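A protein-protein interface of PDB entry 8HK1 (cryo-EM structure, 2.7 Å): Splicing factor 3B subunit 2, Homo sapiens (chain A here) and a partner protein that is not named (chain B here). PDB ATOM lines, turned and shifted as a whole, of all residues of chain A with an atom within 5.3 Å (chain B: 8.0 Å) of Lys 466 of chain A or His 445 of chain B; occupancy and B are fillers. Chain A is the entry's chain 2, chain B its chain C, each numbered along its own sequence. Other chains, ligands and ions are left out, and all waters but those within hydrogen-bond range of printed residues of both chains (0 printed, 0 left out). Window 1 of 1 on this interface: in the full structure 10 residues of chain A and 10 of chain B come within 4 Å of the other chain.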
ATOM      1  N   THR A 461      -1.236  -9.749   8.541  1.00  0.00           N
ATOM      2  CA  THR A 461      -0.113 -10.622   8.254  1.00  0.00           C
ATOM      3  C   THR A 461       1.187  -9.857   8.477  1.00  0.00           C
ATOM      4  O   THR A 461       1.200  -8.628   8.583  1.00  0.00           O
ATOM      5  CB  THR A 461      -0.181 -11.155   6.821  1.00  0.00           C
ATOM      6  OG1 THR A 461       0.181 -10.117   5.902  1.00  0.00           O
ATOM      7  CG2 THR A 461      -1.582 -11.654   6.497  1.00  0.00           C
ATOM      8  N   VAL A 462       2.290 -10.601   8.560  1.00  0.00           N
ATOM      9  CA  VAL A 462       3.576  -9.976   8.860  1.00  0.00           C
ATOM     10  C   VAL A 462       3.937  -8.952   7.792  1.00  0.00           C
ATOM     11  O   VAL A 462       4.345  -7.827   8.102  1.00  0.00           O
ATOM     12  CB  VAL A 462       4.668 -11.050   9.011  1.00  0.00           C
ATOM     13  CG1 VAL A 462       6.043 -10.411   9.022  1.00  0.00           C
ATOM     14  CG2 VAL A 462       4.448 -11.844  10.281  1.00  0.00           C
ATOM     15  N   ALA A 463       3.767  -9.315   6.517  1.00  0.00           N
ATOM     16  CA  ALA A 463       4.120  -8.396   5.440  1.00  0.00           C
ATOM     17  C   ALA A 463       3.157  -7.222   5.375  1.00  0.00           C
ATOM     18  O   ALA A 463       3.547  -6.109   5.005  1.00  0.00           O
ATOM     19  CB  ALA A 463       4.149  -9.143   4.106  1.00  0.00           C
ATOM     20  N   GLU A 464       1.888  -7.448   5.722  1.00  0.00           N
ATOM     21  CA  GLU A 464       0.919  -6.359   5.714  1.00  0.00           C
ATOM     22  C   GLU A 464       1.204  -5.354   6.823  1.00  0.00           C
ATOM     23  O   GLU A 464       1.086  -4.141   6.618  1.00  0.00           O
ATOM     24  CB  GLU A 464      -0.497  -6.918   5.844  1.00  0.00           C
ATOM     25  CG  GLU A 464      -1.572  -5.858   6.012  1.00  0.00           C
ATOM     26  CD  GLU A 464      -2.961  -6.454   6.118  1.00  0.00           C
ATOM     27  OE1 GLU A 464      -3.077  -7.696   6.128  1.00  0.00           O
ATOM     28  OE2 GLU A 464      -3.937  -5.677   6.190  1.00  0.00           O
ATOM     29  N   LEU A 465       1.583  -5.840   8.007  1.00  0.00           N
ATOM     30  CA  LEU A 465       1.897  -4.934   9.107  1.00  0.00           C
ATOM     31  C   LEU A 465       3.246  -4.260   8.891  1.00  0.00           C
ATOM     32  O   LEU A 465       3.468  -3.135   9.354  1.00  0.00           O
ATOM     33  CB  LEU A 465       1.866  -5.694  10.435  1.00  0.00           C
ATOM     34  CG  LEU A 465       2.440  -5.018  11.682  1.00  0.00           C
ATOM     35  CD1 LEU A 465       1.478  -3.978  12.227  1.00  0.00           C
ATOM     36  CD2 LEU A 465       2.764  -6.051  12.746  1.00  0.00           C
ATOM     37  N   LYS A 466       4.157  -4.926   8.178  1.00  0.00           N
ATOM     38  CA  LYS A 466       5.443  -4.312   7.867  1.00  0.00           C
ATOM     39  C   LYS A 466       5.269  -3.117   6.938  1.00  0.00           C
ATOM     40  O   LYS A 466       6.123  -2.222   6.895  1.00  0.00           O
ATOM     41  CB  LYS A 466       6.377  -5.346   7.241  1.00  0.00           C
ATOM     42  CG  LYS A 466       7.104  -6.228   8.241  1.00  0.00           C
ATOM     43  CD  LYS A 466       8.398  -6.767   7.661  1.00  0.00           C
ATOM     44  CE  LYS A 466       9.280  -7.373   8.738  1.00  0.00           C
ATOM     45  NZ  LYS A 466       8.898  -8.762   9.086  1.00  0.00           N
ATOM     46  N   GLN A 467       4.167  -3.084   6.186  1.00  0.00           N
ATOM     47  CA  GLN A 467       3.924  -1.981   5.261  1.00  0.00           C
ATOM     48  C   GLN A 467       3.349  -0.766   5.978  1.00  0.00           C
ATOM     49  O   GLN A 467       3.435   0.362   5.475  1.00  0.00           O
ATOM     50  CB  GLN A 467       2.978  -2.430   4.148  1.00  0.00           C
ATOM     51  CG  GLN A 467       3.618  -3.322   3.103  1.00  0.00           C
ATOM     52  CD  GLN A 467       4.121  -2.542   1.911  1.00  0.00           C
ATOM     53  OE1 GLN A 467       3.572  -1.497   1.563  1.00  0.00           O
ATOM     54  NE2 GLN A 467       5.167  -3.047   1.273  1.00  0.00           N
ATOM     55  N   LEU A 468       2.737  -0.971   7.145  1.00  0.00           N
ATOM     56  CA  LEU A 468       2.075   0.133   7.833  1.00  0.00           C
ATOM     57  C   LEU A 468       3.029   0.873   8.761  1.00  0.00           C
ATOM     58  O   LEU A 468       2.889   2.084   8.969  1.00  0.00           O
ATOM     59  CB  LEU A 468       0.867  -0.389   8.610  1.00  0.00           C
ATOM     60  CG  LEU A 468      -0.322  -0.863   7.773  1.00  0.00           C
ATOM     61  CD1 LEU A 468      -1.585  -0.920   8.617  1.00  0.00           C
ATOM     62  CD2 LEU A 468      -0.523   0.041   6.565  1.00  0.00           C
ATOM     63  N   VAL A 469       4.006   0.166   9.330  1.00  0.00           N
ATOM     64  CA  VAL A 469       4.813   0.733  10.404  1.00  0.00           C
ATOM     65  C   VAL A 469       5.993   1.506   9.830  1.00  0.00           C
ATOM     66  O   VAL A 469       6.448   1.250   8.707  1.00  0.00           O
ATOM     67  CB  VAL A 469       5.283  -0.379  11.357  1.00  0.00           C
ATOM     68  CG1 VAL A 469       4.086  -1.120  11.918  1.00  0.00           C
ATOM     69  CG2 VAL A 469       6.219  -1.337  10.638  1.00  0.00           C
ATOM     70  N   PRO A 472      10.021  -1.414  10.024  1.00  0.00           N
ATOM     71  CA  PRO A 472       9.568  -2.803   9.847  1.00  0.00           C
ATOM     72  C   PRO A 472      10.512  -3.845  10.416  1.00  0.00           C
ATOM     73  O   PRO A 472      10.103  -5.000  10.579  1.00  0.00           O
ATOM     74  CB  PRO A 472       9.442  -2.934   8.323  1.00  0.00           C
ATOM     75  CG  PRO A 472      10.406  -1.940   7.786  1.00  0.00           C
ATOM     76  CD  PRO A 472      10.448  -0.798   8.758  1.00  0.00           C
ATOM     77  N   ASP A 473      11.759  -3.491  10.739  1.00  0.00           N
ATOM     78  CA  ASP A 473      12.720  -4.513  11.142  1.00  0.00           C
ATOM     79  C   ASP A 473      12.545  -4.908  12.605  1.00  0.00           C
ATOM     80  O   ASP A 473      13.220  -5.821  13.091  1.00  0.00           O
ATOM     81  CB  ASP A 473      14.147  -4.035  10.883  1.00  0.00           C
ATOM     82  CG  ASP A 473      14.396  -2.640  11.409  1.00  0.00           C
ATOM     83  OD1 ASP A 473      13.412  -1.924  11.670  1.00  0.00           O
ATOM     84  OD2 ASP A 473      15.577  -2.263  11.562  1.00  0.00           O
ATOM     85  N   VAL A 475       9.487  -5.742  13.642  1.00  0.00           N
ATOM     86  CA  VAL A 475       8.336  -6.636  13.614  1.00  0.00           C
ATOM     87  C   VAL A 475       8.818  -8.081  13.621  1.00  0.00           C
ATOM     88  O   VAL A 475       9.815  -8.430  12.978  1.00  0.00           O
ATOM     89  CB  VAL A 475       7.462  -6.335  12.385  1.00  0.00           C
ATOM     90  CG1 VAL A 475       6.280  -7.286  12.310  1.00  0.00           C
ATOM     91  CG2 VAL A 475       6.980  -4.896  12.422  1.00  0.00           C
ATOM     92  N   GLN B 423      12.524 -19.947  11.274  1.00  0.00           N
ATOM     93  CA  GLN B 423      12.915 -18.570  11.562  1.00  0.00           C
ATOM     94  C   GLN B 423      14.387 -18.340  11.247  1.00  0.00           C
ATOM     95  O   GLN B 423      14.784 -17.233  10.866  1.00  0.00           O
ATOM     96  CB  GLN B 423      12.619 -18.238  13.023  1.00  0.00           C
ATOM     97  CG  GLN B 423      12.045 -16.846  13.247  1.00  0.00           C
ATOM     98  CD  GLN B 423      13.032 -15.746  12.904  1.00  0.00           C
ATOM     99  OE1 GLN B 423      14.132 -15.689  13.455  1.00  0.00           O
ATOM    100  NE2 GLN B 423      12.642 -14.866  11.990  1.00  0.00           N
ATOM    101  N   MET B 435      17.005 -14.343  -2.468  1.00  0.00           N
ATOM    102  CA  MET B 435      16.778 -12.903  -2.447  1.00  0.00           C
ATOM    103  C   MET B 435      17.650 -12.165  -3.451  1.00  0.00           C
ATOM    104  O   MET B 435      17.214 -11.149  -4.000  1.00  0.00           O
ATOM    105  CB  MET B 435      17.018 -12.345  -1.043  1.00  0.00           C
ATOM    106  CG  MET B 435      15.866 -12.575  -0.081  1.00  0.00           C
ATOM    107  SD  MET B 435      14.586 -11.312  -0.207  1.00  0.00           S
ATOM    108  CE  MET B 435      15.373  -9.948   0.642  1.00  0.00           C
ATOM    109  N   PRO B 441      18.752  -6.804  -0.960  1.00  0.00           N
ATOM    110  CA  PRO B 441      19.694  -7.320   0.040  1.00  0.00           C
ATOM    111  C   PRO B 441      18.980  -8.014   1.190  1.00  0.00           C
ATOM    112  O   PRO B 441      17.801  -7.766   1.457  1.00  0.00           O
ATOM    113  CB  PRO B 441      20.429  -6.061   0.519  1.00  0.00           C
ATOM    114  CG  PRO B 441      19.498  -4.938   0.206  1.00  0.00           C
ATOM    115  CD  PRO B 441      18.792  -5.336  -1.053  1.00  0.00           C
ATOM    116  N   ASN B 442      19.712  -8.891   1.870  1.00  0.00           N
ATOM    117  CA  ASN B 442      19.172  -9.572   3.039  1.00  0.00           C
ATOM    118  C   ASN B 442      19.447  -8.762   4.300  1.00  0.00           C
ATOM    119  O   ASN B 442      20.593  -8.658   4.748  1.00  0.00           O
ATOM    120  CB  ASN B 442      19.781 -10.968   3.167  1.00  0.00           C
ATOM    121  CG  ASN B 442      18.761 -12.067   2.976  1.00  0.00           C
ATOM    122  OD1 ASN B 442      17.628 -11.816   2.573  1.00  0.00           O
ATOM    123  ND2 ASN B 442      19.157 -13.299   3.271  1.00  0.00           N
ATOM    124  N   THR B 443      18.393  -8.189   4.871  1.00  0.00           N
ATOM    125  CA  THR B 443      18.520  -7.416   6.100  1.00  0.00           C
ATOM    126  C   THR B 443      17.422  -7.856   7.057  1.00  0.00           C
ATOM    127  O   THR B 443      16.589  -8.704   6.731  1.00  0.00           O
ATOM    128  CB  THR B 443      18.445  -5.910   5.831  1.00  0.00           C
ATOM    129  OG1 THR B 443      17.507  -5.655   4.778  1.00  0.00           O
ATOM    130  CG2 THR B 443      19.810  -5.369   5.428  1.00  0.00           C
ATOM    131  N   ALA B 444      17.437  -7.264   8.253  1.00  0.00           N
ATOM    132  CA  ALA B 444      16.447  -7.625   9.263  1.00  0.00           C
ATOM    133  C   ALA B 444      15.053  -7.169   8.856  1.00  0.00           C
ATOM    134  O   ALA B 444      14.049  -7.700   9.346  1.00  0.00           O
ATOM    135  CB  ALA B 444      16.836  -7.031  10.614  1.00  0.00           C
ATOM    136  N   HIS B 445      14.968  -6.183   7.960  1.00  0.00           N
ATOM    137  CA  HIS B 445      13.666  -5.733   7.477  1.00  0.00           C
ATOM    138  C   HIS B 445      12.941  -6.842   6.727  1.00  0.00           C
ATOM    139  O   HIS B 445      11.721  -6.989   6.851  1.00  0.00           O
ATOM    140  CB  HIS B 445      13.826  -4.510   6.575  1.00  0.00           C
ATOM    141  CG  HIS B 445      14.671  -3.422   7.163  1.00  0.00           C
ATOM    142  ND1 HIS B 445      14.146  -2.215   7.571  1.00  0.00           N
ATOM    143  CD2 HIS B 445      16.002  -3.351   7.397  1.00  0.00           C
ATOM    144  CE1 HIS B 445      15.118  -1.450   8.040  1.00  0.00           C
ATOM    145  NE2 HIS B 445      16.254  -2.117   7.945  1.00  0.00           N
ATOM    146  N   PHE B 446      13.673  -7.626   5.938  1.00  0.00           N
ATOM    147  CA  PHE B 446      13.072  -8.703   5.150  1.00  0.00           C
ATOM    148  C   PHE B 446      13.224 -10.032   5.891  1.00  0.00           C
ATOM    149  O   PHE B 446      13.889 -10.968   5.444  1.00  0.00           O
ATOM    150  CB  PHE B 446      13.689  -8.752   3.760  1.00  0.00           C
ATOM    151  CG  PHE B 446      13.467  -7.502   2.963  1.00  0.00           C
ATOM    152  CD1 PHE B 446      12.266  -7.285   2.313  1.00  0.00           C
ATOM    153  CD2 PHE B 446      14.453  -6.534   2.877  1.00  0.00           C
ATOM    154  CE1 PHE B 446      12.054  -6.133   1.582  1.00  0.00           C
ATOM    155  CE2 PHE B 446      14.249  -5.380   2.150  1.00  0.00           C
ATOM    156  CZ  PHE B 446      13.048  -5.180   1.502  1.00  0.00           C
ATOM    157  N   ALA B 447      12.584 -10.093   7.054  1.00  0.00           N
ATOM    158  CA  ALA B 447      12.491 -11.312   7.834  1.00  0.00           C
ATOM    159  C   ALA B 447      11.023 -11.664   8.016  1.00  0.00           C
ATOM    160  O   ALA B 447      10.160 -10.784   8.090  1.00  0.00           O
ATOM    161  CB  ALA B 447      13.181 -11.170   9.195  1.00  0.00           C
ATOM    162  N   ASN B 448      10.747 -12.969   8.066  1.00  0.00           N
ATOM    163  CA  ASN B 448       9.384 -13.494   8.149  1.00  0.00           C
ATOM    164  C   ASN B 448       8.539 -13.081   6.944  1.00  0.00           C
ATOM    165  O   ASN B 448       7.310 -13.154   6.979  1.00  0.00           O
ATOM    166  CB  ASN B 448       8.700 -13.079   9.454  1.00  0.00           C
ATOM    167  CG  ASN B 448       9.539 -13.390  10.675  1.00  0.00           C
ATOM    168  OD1 ASN B 448      10.289 -12.544  11.163  1.00  0.00           O
ATOM    169  ND2 ASN B 448       9.418 -14.612  11.179  1.00  0.00           N
ATOM    170  N   VAL B 449       9.194 -12.643   5.871  1.00  0.00           N
ATOM    171  CA  VAL B 449       8.533 -12.323   4.610  1.00  0.00           C
ATOM    172  C   VAL B 449       8.885 -13.410   3.608  1.00  0.00           C
ATOM    173  O   VAL B 449      10.060 -13.586   3.259  1.00  0.00           O
ATOM    174  CB  VAL B 449       8.955 -10.937   4.095  1.00  0.00           C
ATOM    175  CG1 VAL B 449       8.483 -10.734   2.665  1.00  0.00           C
ATOM    176  CG2 VAL B 449       8.409  -9.847   5.003  1.00  0.00           C
ATOM    177  N   ASP B 454       5.354  -9.246  -2.034  1.00  0.00           N
ATOM    178  CA  ASP B 454       5.464  -8.540  -0.763  1.00  0.00           C
ATOM    179  C   ASP B 454       6.876  -8.007  -0.567  1.00  0.00           C
ATOM    180  O   ASP B 454       7.064  -6.865  -0.131  1.00  0.00           O
ATOM    181  CB  ASP B 454       5.076  -9.463   0.390  1.00  0.00           C
ATOM    182  CG  ASP B 454       3.578  -9.643   0.511  1.00  0.00           C
ATOM    183  OD1 ASP B 454       2.829  -8.770   0.026  1.00  0.00           O
ATOM    184  OD2 ASP B 454       3.148 -10.662   1.091  1.00  0.00           O
ATOM    185  N   LEU B 458       7.817  -4.050  -0.292  1.00  0.00           N
ATOM    186  CA  LEU B 458       8.485  -3.522   0.891  1.00  0.00           C
ATOM    187  C   LEU B 458       9.842  -2.932   0.528  1.00  0.00           C
ATOM    188  O   LEU B 458      10.301  -1.972   1.160  1.00  0.00           O
ATOM    189  CB  LEU B 458       8.628  -4.617   1.946  1.00  0.00           C
ATOM    190  CG  LEU B 458       9.048  -4.164   3.345  1.00  0.00           C
ATOM    191  CD1 LEU B 458       7.854  -3.588   4.089  1.00  0.00           C
ATOM    192  CD2 LEU B 458       9.660  -5.315   4.119  1.00  0.00           C
ATOM    193  N   TRP B 459      10.485  -3.470  -0.511  1.00  0.00           N
ATOM    194  CA  TRP B 459      11.735  -2.889  -0.979  1.00  0.00           C
ATOM    195  C   TRP B 459      11.503  -1.524  -1.611  1.00  0.00           C
ATOM    196  O   TRP B 459      12.282  -0.592  -1.389  1.00  0.00           O
ATOM    197  CB  TRP B 459      12.418  -3.830  -1.970  1.00  0.00           C
ATOM    198  CG  TRP B 459      13.679  -3.271  -2.546  1.00  0.00           C
ATOM    199  CD1 TRP B 459      13.935  -3.019  -3.861  1.00  0.00           C
ATOM    200  CD2 TRP B 459      14.858  -2.886  -1.827  1.00  0.00           C
ATOM    201  NE1 TRP B 459      15.199  -2.505  -4.007  1.00  0.00           N
ATOM    202  CE2 TRP B 459      15.787  -2.414  -2.774  1.00  0.00           C
ATOM    203  CE3 TRP B 459      15.217  -2.901  -0.476  1.00  0.00           C
ATOM    204  CZ2 TRP B 459      17.051  -1.957  -2.413  1.00  0.00           C
ATOM    205  CZ3 TRP B 459      16.473  -2.447  -0.121  1.00  0.00           C
ATOM    206  CH2 TRP B 459      17.376  -1.982  -1.084  1.00  0.00           C
ATOM    207  N   LYS B 461       9.101   0.480  -0.776  1.00  0.00           N
ATOM    208  CA  LYS B 461       8.816   1.358   0.356  1.00  0.00           C
ATOM    209  C   LYS B 461      10.095   1.798   1.063  1.00  0.00           C
ATOM    210  O   LYS B 461      10.284   2.991   1.338  1.00  0.00           O
ATOM    211  CB  LYS B 461       7.890   0.652   1.343  1.00  0.00           C
ATOM    212  CG  LYS B 461       7.514   1.502   2.541  1.00  0.00           C
ATOM    213  CD  LYS B 461       6.218   1.030   3.165  1.00  0.00           C
ATOM    214  CE  LYS B 461       6.445   0.612   4.612  1.00  0.00           C
ATOM    215  NZ  LYS B 461       6.409   1.767   5.549  1.00  0.00           N
ATOM    216  N   LEU B 462      10.972   0.845   1.384  1.00  0.00           N
ATOM    217  CA  LEU B 462      12.204   1.177   2.093  1.00  0.00           C
ATOM    218  C   LEU B 462      13.107   2.062   1.246  1.00  0.00           C
ATOM    219  O   LEU B 462      13.754   2.982   1.766  1.00  0.00           O
ATOM    220  CB  LEU B 462      12.935  -0.103   2.493  1.00  0.00           C
ATOM    221  CG  LEU B 462      12.460  -0.770   3.783  1.00  0.00           C
ATOM    222  CD1 LEU B 462      13.157  -2.104   3.973  1.00  0.00           C
ATOM    223  CD2 LEU B 462      12.691   0.136   4.984  1.00  0.00           C
ATOM    224  N   GLN B 465      11.653   5.595   1.384  1.00  0.00           N
ATOM    225  CA  GLN B 465      11.940   6.175   2.695  1.00  0.00           C
ATOM    226  C   GLN B 465      13.391   6.626   2.823  1.00  0.00           C
ATOM    227  O   GLN B 465      13.656   7.803   3.119  1.00  0.00           O
ATOM    228  CB  GLN B 465      11.628   5.153   3.788  1.00  0.00           C
ATOM    229  CG  GLN B 465      11.417   5.747   5.168  1.00  0.00           C
ATOM    230  CD  GLN B 465      11.503   4.701   6.261  1.00  0.00           C
ATOM    231  OE1 GLN B 465      12.352   4.782   7.147  1.00  0.00           O
ATOM    232  NE2 GLN B 465      10.625   3.706   6.200  1.00  0.00           N
ATOM    233  N   LYS B 466      14.343   5.714   2.603  1.00  0.00           N
ATOM    234  CA  LYS B 466      15.744   6.060   2.794  1.00  0.00           C
ATOM    235  C   LYS B 466      16.186   7.137   1.814  1.00  0.00           C
ATOM    236  O   LYS B 466      16.796   8.134   2.217  1.00  0.00           O
ATOM    237  CB  LYS B 466      16.622   4.813   2.674  1.00  0.00           C
ATOM    238  CG  LYS B 466      17.058   4.263   4.025  1.00  0.00           C
ATOM    239  CD  LYS B 466      17.809   2.949   3.900  1.00  0.00           C
ATOM    240  CE  LYS B 466      16.986   1.888   3.185  1.00  0.00           C
ATOM    241  NZ  LYS B 466      17.845   0.776   2.683  1.00  0.00           N
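NZ of Lys 461 of chain B lies close to O of Gln 467 of chain A.
O of Ala 447 of chain B lies within hydrogen-bond range of NZ of Lys 466 of chain A (2.6 Å).
NZ of Lys 461 of chain B is in hydrogen-bond range of O of Val 469 of chain A, 3.2 Å away.
NE2 of Gln 467 of chain A sits close to N of Leu 458 of chain B (3.2 Å).
NE2 of Gln 423 of chain B lies close to ND2 of Asn 448 of chain B (3.3 Å).
Asn 448 of chain B touches Val 462 of chain A (O to CG1, 3.6 Å).
CB of Ala 463 of chain A touches OD2 of Asp 454 of chain B, 3.5 Å away.
O of His 445 of chain B touches CE of Lys 466 of chain A (3.1 Å).
Leu 458 of chain B touches Lys 466 of chain A (CD1 to O, 3.6 Å).
Lys 466 of chain A touches Lys 461 of chain B (O to CE, 3.7 Å).
Pro 472 of chain A touches His 445 of chain B (CG to ND1, 3.8 Å).
Asp 473 of chain A touches Ala 444 of chain B.
Asp 473 of chain A touches His 445 of chain B.
Of chain A, only Lys 466, Pro 472 and Asp 473 come within 4 Å of His 445 of chain B.
Of the printed residues of chain B, Asp 473 of chain A touches Ala 444 (3.8 Å) and His 445 (3.6 Å).
Of the printed residues of chain B, Val 469 of chain A touches Lys 461.
Of the printed residues of chain A, Ala 444 of chain B touches Asp 473.
Met 435 of chain B touches none of the printed residues of chain A.
The nearest printed residue of chain A that does not touch His 445 of chain B is Val 475 of chain A (6.6 Å).
The nearest printed residue of chain B that does not touch Gln 467 of chain A is Asp 454 of chain B (4.5 Å).
Printed residues of chain B that touch a printed residue of chain A: Ala 444, His 445, Ala 447, Asn 448, Asp 454, Leu 458 and Lys 461.
Hydrophobic or aromatic side chains of chain B that line the printed part of chain A: His 445 and Leu 458.
Hydrophobic or aromatic side chains of chain A within 4 Å of the printed part of chain B: Val 462, Ala 463 and Pro 472.
Among the printed residues, no Asp or Glu carboxylate lies within 4 Å of a Lys or Arg side-chain nitrogen of the other chain.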
